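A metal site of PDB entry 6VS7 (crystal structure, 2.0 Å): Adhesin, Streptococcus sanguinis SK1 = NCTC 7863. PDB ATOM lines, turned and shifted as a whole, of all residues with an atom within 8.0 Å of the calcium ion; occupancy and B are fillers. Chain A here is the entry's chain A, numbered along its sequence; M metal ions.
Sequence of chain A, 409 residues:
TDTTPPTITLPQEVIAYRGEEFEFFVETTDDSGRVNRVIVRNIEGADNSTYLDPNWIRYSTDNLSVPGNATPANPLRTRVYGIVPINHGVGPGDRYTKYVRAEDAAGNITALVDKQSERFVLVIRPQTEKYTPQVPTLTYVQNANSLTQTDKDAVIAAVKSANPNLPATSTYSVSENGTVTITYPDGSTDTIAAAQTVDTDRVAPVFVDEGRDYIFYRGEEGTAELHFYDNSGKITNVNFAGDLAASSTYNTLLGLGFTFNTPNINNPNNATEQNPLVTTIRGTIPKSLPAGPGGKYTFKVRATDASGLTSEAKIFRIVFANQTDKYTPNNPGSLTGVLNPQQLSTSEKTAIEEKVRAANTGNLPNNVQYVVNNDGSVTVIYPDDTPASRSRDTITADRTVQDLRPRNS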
ATOM      1  N   TYR A 140       4.827 -12.014 -26.205  1.00  0.00           N
ATOM      2  CA  TYR A 140       5.197 -10.778 -25.513  1.00  0.00           C
ATOM      3  C   TYR A 140       6.162 -10.003 -26.397  1.00  0.00           C
ATOM      4  O   TYR A 140       7.264 -10.483 -26.685  1.00  0.00           O
ATOM      5  CB  TYR A 140       5.805 -11.079 -24.146  1.00  0.00           C
ATOM      6  CG  TYR A 140       4.754 -11.445 -23.144  1.00  0.00           C
ATOM      7  CD1 TYR A 140       4.038 -10.461 -22.477  1.00  0.00           C
ATOM      8  CD2 TYR A 140       4.420 -12.776 -22.913  1.00  0.00           C
ATOM      9  CE1 TYR A 140       3.036 -10.798 -21.572  1.00  0.00           C
ATOM     10  CE2 TYR A 140       3.420 -13.129 -22.027  1.00  0.00           C
ATOM     11  CZ  TYR A 140       2.745 -12.131 -21.345  1.00  0.00           C
ATOM     12  OH  TYR A 140       1.753 -12.483 -20.452  1.00  0.00           O
ATOM     13  N   VAL A 141       5.740  -8.825 -26.816  1.00  0.00           N
ATOM     14  CA  VAL A 141       6.449  -8.067 -27.835  1.00  0.00           C
ATOM     15  C   VAL A 141       6.895  -6.727 -27.250  1.00  0.00           C
ATOM     16  O   VAL A 141       6.394  -6.268 -26.225  1.00  0.00           O
ATOM     17  CB  VAL A 141       5.581  -7.844 -29.099  1.00  0.00           C
ATOM     18  CG1 VAL A 141       5.065  -9.151 -29.620  1.00  0.00           C
ATOM     19  CG2 VAL A 141       4.427  -6.933 -28.787  1.00  0.00           C
ATOM     20  N   THR A 200       2.402  -6.177 -24.771  1.00  0.00           N
ATOM     21  CA  THR A 200       3.744  -5.625 -24.670  1.00  0.00           C
ATOM     22  C   THR A 200       4.436  -6.202 -23.441  1.00  0.00           C
ATOM     23  O   THR A 200       3.814  -6.448 -22.397  1.00  0.00           O
ATOM     24  CB  THR A 200       3.684  -4.095 -24.663  1.00  0.00           C
ATOM     25  OG1 THR A 200       4.822  -3.547 -23.978  1.00  0.00           O
ATOM     26  CG2 THR A 200       2.395  -3.609 -24.049  1.00  0.00           C
ATOM     27  N   ASP A 201       5.705  -6.535 -23.592  1.00  0.00           N
ATOM     28  CA  ASP A 201       6.449  -7.124 -22.496  1.00  0.00           C
ATOM     29  C   ASP A 201       6.779  -6.016 -21.484  1.00  0.00           C
ATOM     30  O   ASP A 201       7.535  -5.097 -21.787  1.00  0.00           O
ATOM     31  CB  ASP A 201       7.712  -7.801 -23.003  1.00  0.00           C
ATOM     32  CG  ASP A 201       8.296  -8.760 -21.990  1.00  0.00           C
ATOM     33  OD1 ASP A 201       8.148  -8.506 -20.770  1.00  0.00           O
ATOM     34  OD2 ASP A 201       8.870  -9.778 -22.414  1.00  0.00           O
ATOM     35  N   ARG A 202       6.193  -6.111 -20.294  1.00  0.00           N
ATOM     36  CA  ARG A 202       6.384  -5.116 -19.240  1.00  0.00           C
ATOM     37  C   ARG A 202       7.165  -5.629 -18.046  1.00  0.00           C
ATOM     38  O   ARG A 202       7.281  -4.912 -17.045  1.00  0.00           O
ATOM     39  CB  ARG A 202       5.034  -4.600 -18.751  1.00  0.00           C
ATOM     40  CG  ARG A 202       4.435  -3.497 -19.560  1.00  0.00           C
ATOM     41  CD  ARG A 202       3.052  -3.193 -19.017  1.00  0.00           C
ATOM     42  NE  ARG A 202       2.113  -4.271 -19.296  1.00  0.00           N
ATOM     43  CZ  ARG A 202       1.621  -5.135 -18.403  1.00  0.00           C
ATOM     44  NH1 ARG A 202       1.958  -5.046 -17.117  1.00  0.00           N
ATOM     45  NH2 ARG A 202       0.774  -6.076 -18.806  1.00  0.00           N
ATOM     46  N   VAL A 203       7.670  -6.861 -18.094  1.00  0.00           N
ATOM     47  CA  VAL A 203       8.311  -7.486 -16.945  1.00  0.00           C
ATOM     48  C   VAL A 203       9.705  -7.958 -17.331  1.00  0.00           C
ATOM     49  O   VAL A 203       9.868  -8.672 -18.327  1.00  0.00           O
ATOM     50  CB  VAL A 203       7.487  -8.657 -16.389  1.00  0.00           C
ATOM     51  CG1 VAL A 203       8.066  -9.118 -15.059  1.00  0.00           C
ATOM     52  CG2 VAL A 203       6.023  -8.261 -16.228  1.00  0.00           C
ATOM     53  N   ALA A 204      10.701  -7.565 -16.560  1.00  0.00           N
ATOM     54  CA  ALA A 204      12.048  -7.973 -16.861  1.00  0.00           C
ATOM     55  C   ALA A 204      12.282  -9.400 -16.354  1.00  0.00           C
ATOM     56  O   ALA A 204      11.526  -9.902 -15.521  1.00  0.00           O
ATOM     57  CB  ALA A 204      13.037  -6.989 -16.241  1.00  0.00           C
ATOM     58  N   PRO A 205      13.284 -10.090 -16.887  1.00  0.00           N
ATOM     59  CA  PRO A 205      13.633 -11.416 -16.367  1.00  0.00           C
ATOM     60  C   PRO A 205      13.845 -11.434 -14.859  1.00  0.00           C
ATOM     61  O   PRO A 205      14.135 -10.406 -14.241  1.00  0.00           O
ATOM     62  CB  PRO A 205      14.932 -11.738 -17.131  1.00  0.00           C
ATOM     63  CG  PRO A 205      14.754 -11.038 -18.442  1.00  0.00           C
ATOM     64  CD  PRO A 205      14.079  -9.733 -18.084  1.00  0.00           C
ATOM     65  N   VAL A 206      13.660 -12.601 -14.248  1.00  0.00           N
ATOM     66  CA  VAL A 206      13.800 -12.773 -12.804  1.00  0.00           C
ATOM     67  C   VAL A 206      15.033 -13.639 -12.545  1.00  0.00           C
ATOM     68  O   VAL A 206      15.234 -14.658 -13.213  1.00  0.00           O
ATOM     69  CB  VAL A 206      12.535 -13.405 -12.192  1.00  0.00           C
ATOM     70  CG1 VAL A 206      12.698 -13.659 -10.705  1.00  0.00           C
ATOM     71  CG2 VAL A 206      11.314 -12.522 -12.449  1.00  0.00           C
ATOM     72  N   TYR A 229      14.306 -16.807 -15.249  1.00  0.00           N
ATOM     73  CA  TYR A 229      13.161 -17.006 -16.128  1.00  0.00           C
ATOM     74  C   TYR A 229      12.627 -15.640 -16.548  1.00  0.00           C
ATOM     75  O   TYR A 229      13.044 -14.595 -16.038  1.00  0.00           O
ATOM     76  CB  TYR A 229      12.050 -17.859 -15.477  1.00  0.00           C
ATOM     77  CG  TYR A 229      11.322 -17.195 -14.323  1.00  0.00           C
ATOM     78  CD1 TYR A 229      10.185 -16.410 -14.544  1.00  0.00           C
ATOM     79  CD2 TYR A 229      11.753 -17.356 -13.006  1.00  0.00           C
ATOM     80  CE1 TYR A 229       9.512 -15.802 -13.484  1.00  0.00           C
ATOM     81  CE2 TYR A 229      11.101 -16.753 -11.940  1.00  0.00           C
ATOM     82  CZ  TYR A 229       9.970 -15.974 -12.182  1.00  0.00           C
ATOM     83  OH  TYR A 229       9.319 -15.364 -11.132  1.00  0.00           O
ATOM     84  N   ASP A 230      11.694 -15.667 -17.501  1.00  0.00           N
ATOM     85  CA  ASP A 230      11.045 -14.455 -17.982  1.00  0.00           C
ATOM     86  C   ASP A 230       9.589 -14.752 -18.300  1.00  0.00           C
ATOM     87  O   ASP A 230       9.252 -15.861 -18.724  1.00  0.00           O
ATOM     88  CB  ASP A 230      11.733 -13.891 -19.227  1.00  0.00           C
ATOM     89  CG  ASP A 230      11.158 -12.543 -19.632  1.00  0.00           C
ATOM     90  OD1 ASP A 230      11.345 -11.590 -18.859  1.00  0.00           O
ATOM     91  OD2 ASP A 230      10.504 -12.446 -20.692  1.00  0.00           O
ATOM     92  N   ASN A 231       8.737 -13.735 -18.108  1.00  0.00           N
ATOM     93  CA  ASN A 231       7.324 -13.897 -18.436  1.00  0.00           C
ATOM     94  C   ASN A 231       7.111 -14.301 -19.893  1.00  0.00           C
ATOM     95  O   ASN A 231       6.116 -14.952 -20.219  1.00  0.00           O
ATOM     96  CB  ASN A 231       6.540 -12.613 -18.108  1.00  0.00           C
ATOM     97  CG  ASN A 231       6.954 -11.411 -18.956  1.00  0.00           C
ATOM     98  OD1 ASN A 231       8.129 -11.203 -19.255  1.00  0.00           O
ATOM     99  ND2 ASN A 231       5.983 -10.598 -19.327  1.00  0.00           N
ATOM    100  N   SER A 232       8.035 -13.958 -20.771  1.00  0.00           N
ATOM    101  CA  SER A 232       7.914 -14.383 -22.165  1.00  0.00           C
ATOM    102  C   SER A 232       8.382 -15.816 -22.393  1.00  0.00           C
ATOM    103  O   SER A 232       8.135 -16.358 -23.477  1.00  0.00           O
ATOM    104  CB  SER A 232       8.726 -13.466 -23.066  1.00  0.00           C
ATOM    105  OG  SER A 232      10.116 -13.659 -22.836  1.00  0.00           O
ATOM    106  N   GLY A 233       9.060 -16.419 -21.433  1.00  0.00           N
ATOM    107  CA  GLY A 233       9.694 -17.700 -21.640  1.00  0.00           C
ATOM    108  C   GLY A 233      11.048 -17.662 -22.295  1.00  0.00           C
ATOM    109  O   GLY A 233      11.644 -18.726 -22.523  1.00  0.00           O
ATOM    110  N   LYS A 234      11.581 -16.482 -22.590  1.00  0.00           N
ATOM    111  CA  LYS A 234      12.765 -16.377 -23.426  1.00  0.00           C
ATOM    112  C   LYS A 234      13.684 -15.290 -22.901  1.00  0.00           C
ATOM    113  O   LYS A 234      13.270 -14.139 -22.735  1.00  0.00           O
ATOM    114  CB  LYS A 234      12.367 -16.075 -24.876  1.00  0.00           C
ATOM    115  CG  LYS A 234      13.522 -15.690 -25.767  1.00  0.00           C
ATOM    116  CD  LYS A 234      14.518 -16.823 -25.933  1.00  0.00           C
ATOM    117  CE  LYS A 234      15.679 -16.363 -26.812  1.00  0.00           C
ATOM    118  NZ  LYS A 234      16.834 -17.303 -26.785  1.00  0.00           N
ATOM    119  N   ILE A 235      14.945 -15.662 -22.674  1.00  0.00           N
ATOM    120  CA  ILE A 235      15.999 -14.738 -22.292  1.00  0.00           C
ATOM    121  C   ILE A 235      17.075 -14.796 -23.361  1.00  0.00           C
ATOM    122  O   ILE A 235      17.453 -15.886 -23.811  1.00  0.00           O
ATOM    123  CB  ILE A 235      16.581 -15.058 -20.897  1.00  0.00           C
ATOM    124  CG1 ILE A 235      15.624 -14.583 -19.816  1.00  0.00           C
ATOM    125  CG2 ILE A 235      17.990 -14.459 -20.746  1.00  0.00           C
ATOM    126  CD1 ILE A 235      15.806 -15.275 -18.464  1.00  0.00           C
ATOM    127  N   ALA A 303      19.775  -9.845 -16.667  1.00  0.00           N
ATOM    128  CA  ALA A 303      19.305 -10.645 -17.788  1.00  0.00           C
ATOM    129  C   ALA A 303      18.356  -9.832 -18.646  1.00  0.00           C
ATOM    130  O   ALA A 303      17.533  -9.076 -18.127  1.00  0.00           O
ATOM    131  CB  ALA A 303      18.609 -11.931 -17.306  1.00  0.00           C
ATOM    132  N   THR A 304      18.430 -10.059 -19.931  1.00  0.00           N
ATOM    133  CA  THR A 304      17.660  -9.361 -20.903  1.00  0.00           C
ATOM    134  C   THR A 304      16.742 -10.250 -21.716  1.00  0.00           C
ATOM    135  O   THR A 304      17.156 -11.291 -22.143  1.00  0.00           O
ATOM    136  CB  THR A 304      18.667  -8.701 -21.825  1.00  0.00           C
ATOM    137  OG1 THR A 304      19.333  -7.704 -21.101  1.00  0.00           O
ATOM    138  CG2 THR A 304      18.021  -8.079 -22.893  1.00  0.00           C
ATOM    139  N   ASP A 305      15.493  -9.863 -21.911  1.00  0.00           N
ATOM    140  CA  ASP A 305      14.615 -10.687 -22.719  1.00  0.00           C
ATOM    141  C   ASP A 305      14.681 -10.236 -24.194  1.00  0.00           C
ATOM    142  O   ASP A 305      15.396  -9.298 -24.555  1.00  0.00           O
ATOM    143  CB  ASP A 305      13.181 -10.685 -22.167  1.00  0.00           C
ATOM    144  CG  ASP A 305      12.523  -9.290 -22.090  1.00  0.00           C
ATOM    145  OD1 ASP A 305      12.782  -8.421 -22.950  1.00  0.00           O
ATOM    146  OD2 ASP A 305      11.699  -9.095 -21.157  1.00  0.00           O
ATOM    147  N   ALA A 306      13.954 -10.953 -25.058  1.00  0.00           N
ATOM    148  CA  ALA A 306      14.005 -10.670 -26.497  1.00  0.00           C
ATOM    149  C   ALA A 306      13.388  -9.322 -26.856  1.00  0.00           C
ATOM    150  O   ALA A 306      13.701  -8.780 -27.928  1.00  0.00           O
ATOM    151  CB  ALA A 306      13.313 -11.789 -27.274  1.00  0.00           C
ATOM    152  N   SER A 307      12.537  -8.758 -26.004  1.00  0.00           N
ATOM    153  CA  SER A 307      12.033  -7.409 -26.234  1.00  0.00           C
ATOM    154  C   SER A 307      12.953  -6.316 -25.725  1.00  0.00           C
ATOM    155  O   SER A 307      12.625  -5.143 -25.875  1.00  0.00           O
ATOM    156  CB  SER A 307      10.668  -7.241 -25.570  1.00  0.00           C
ATOM    157  OG  SER A 307      10.875  -7.045 -24.194  1.00  0.00           O
ATOM    158  N   GLY A 308      14.070  -6.665 -25.100  1.00  0.00           N
ATOM    159  CA  GLY A 308      15.060  -5.686 -24.688  1.00  0.00           C
ATOM    160  C   GLY A 308      14.923  -5.189 -23.272  1.00  0.00           C
ATOM    161  O   GLY A 308      15.708  -4.317 -22.865  1.00  0.00           O
ATOM    162  N   LEU A 309      13.959  -5.696 -22.509  1.00  0.00           N
ATOM    163  CA  LEU A 309      13.903  -5.389 -21.090  1.00  0.00           C
ATOM    164  C   LEU A 309      15.066  -6.075 -20.356  1.00  0.00           C
ATOM    165  O   LEU A 309      15.267  -7.281 -20.499  1.00  0.00           O
ATOM    166  CB  LEU A 309      12.571  -5.860 -20.500  1.00  0.00           C
ATOM    167  CG  LEU A 309      11.505  -4.797 -20.349  1.00  0.00           C
ATOM    168  CD1 LEU A 309      10.314  -5.355 -19.607  1.00  0.00           C
ATOM    169  CD2 LEU A 309      12.098  -3.604 -19.638  1.00  0.00           C
ATOM    170  N   THR A 310      15.823  -5.315 -19.597  1.00  0.00           N
ATOM    171  CA  THR A 310      16.916  -5.850 -18.837  1.00  0.00           C
ATOM    172  C   THR A 310      16.559  -5.742 -17.381  1.00  0.00           C
ATOM    173  O   THR A 310      16.173  -4.712 -16.925  1.00  0.00           O
ATOM    174  CB  THR A 310      18.189  -5.061 -19.076  1.00  0.00           C
ATOM    175  OG1 THR A 310      18.543  -5.104 -20.436  1.00  0.00           O
ATOM    176  CG2 THR A 310      19.295  -5.578 -18.270  1.00  0.00           C
HETATM  177 CA    CA M   1       9.876 -10.001 -20.110  1.00  0.00          CA
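OD1 of Asp 305 lies within hydrogen-bond range of N of Leu 309 (3.0 Å).
OD1 of Asp 305 is in hydrogen-bond range of OG of Ser 307 (2.7 Å).
The side-chain carboxylate (OD1) of Asp 305 lies within hydrogen-bond range of the backbone NH (N) of Gly 308, at 3.1 Å.
The backbone NH (N) of Asp 201 is in hydrogen-bond range of the backbone carbonyl oxygen (O) of Val 141.
The side-chain hydroxyl (OG) of Ser 232 lies close to the side-chain carboxylate (OD2) of Asp 230, at 2.5 Å.
The nearest printed residue that does not touch the calcium ion is Ala 204 (4.4 Å).
The calcium ion is bound by the backbone carbonyl oxygen (O) of Val 203, the side-chain amide oxygen (OD1) of Asn 231, the side-chain carboxylate (OD2) of Asp 305, the side-chain carboxylate (OD1) of Asp 201, the side-chain carboxylate (OD1) of Asp 230, the side-chain carboxylate (OD2) of Asp 201 and the side-chain carboxylate (OD2) of Asp 230.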
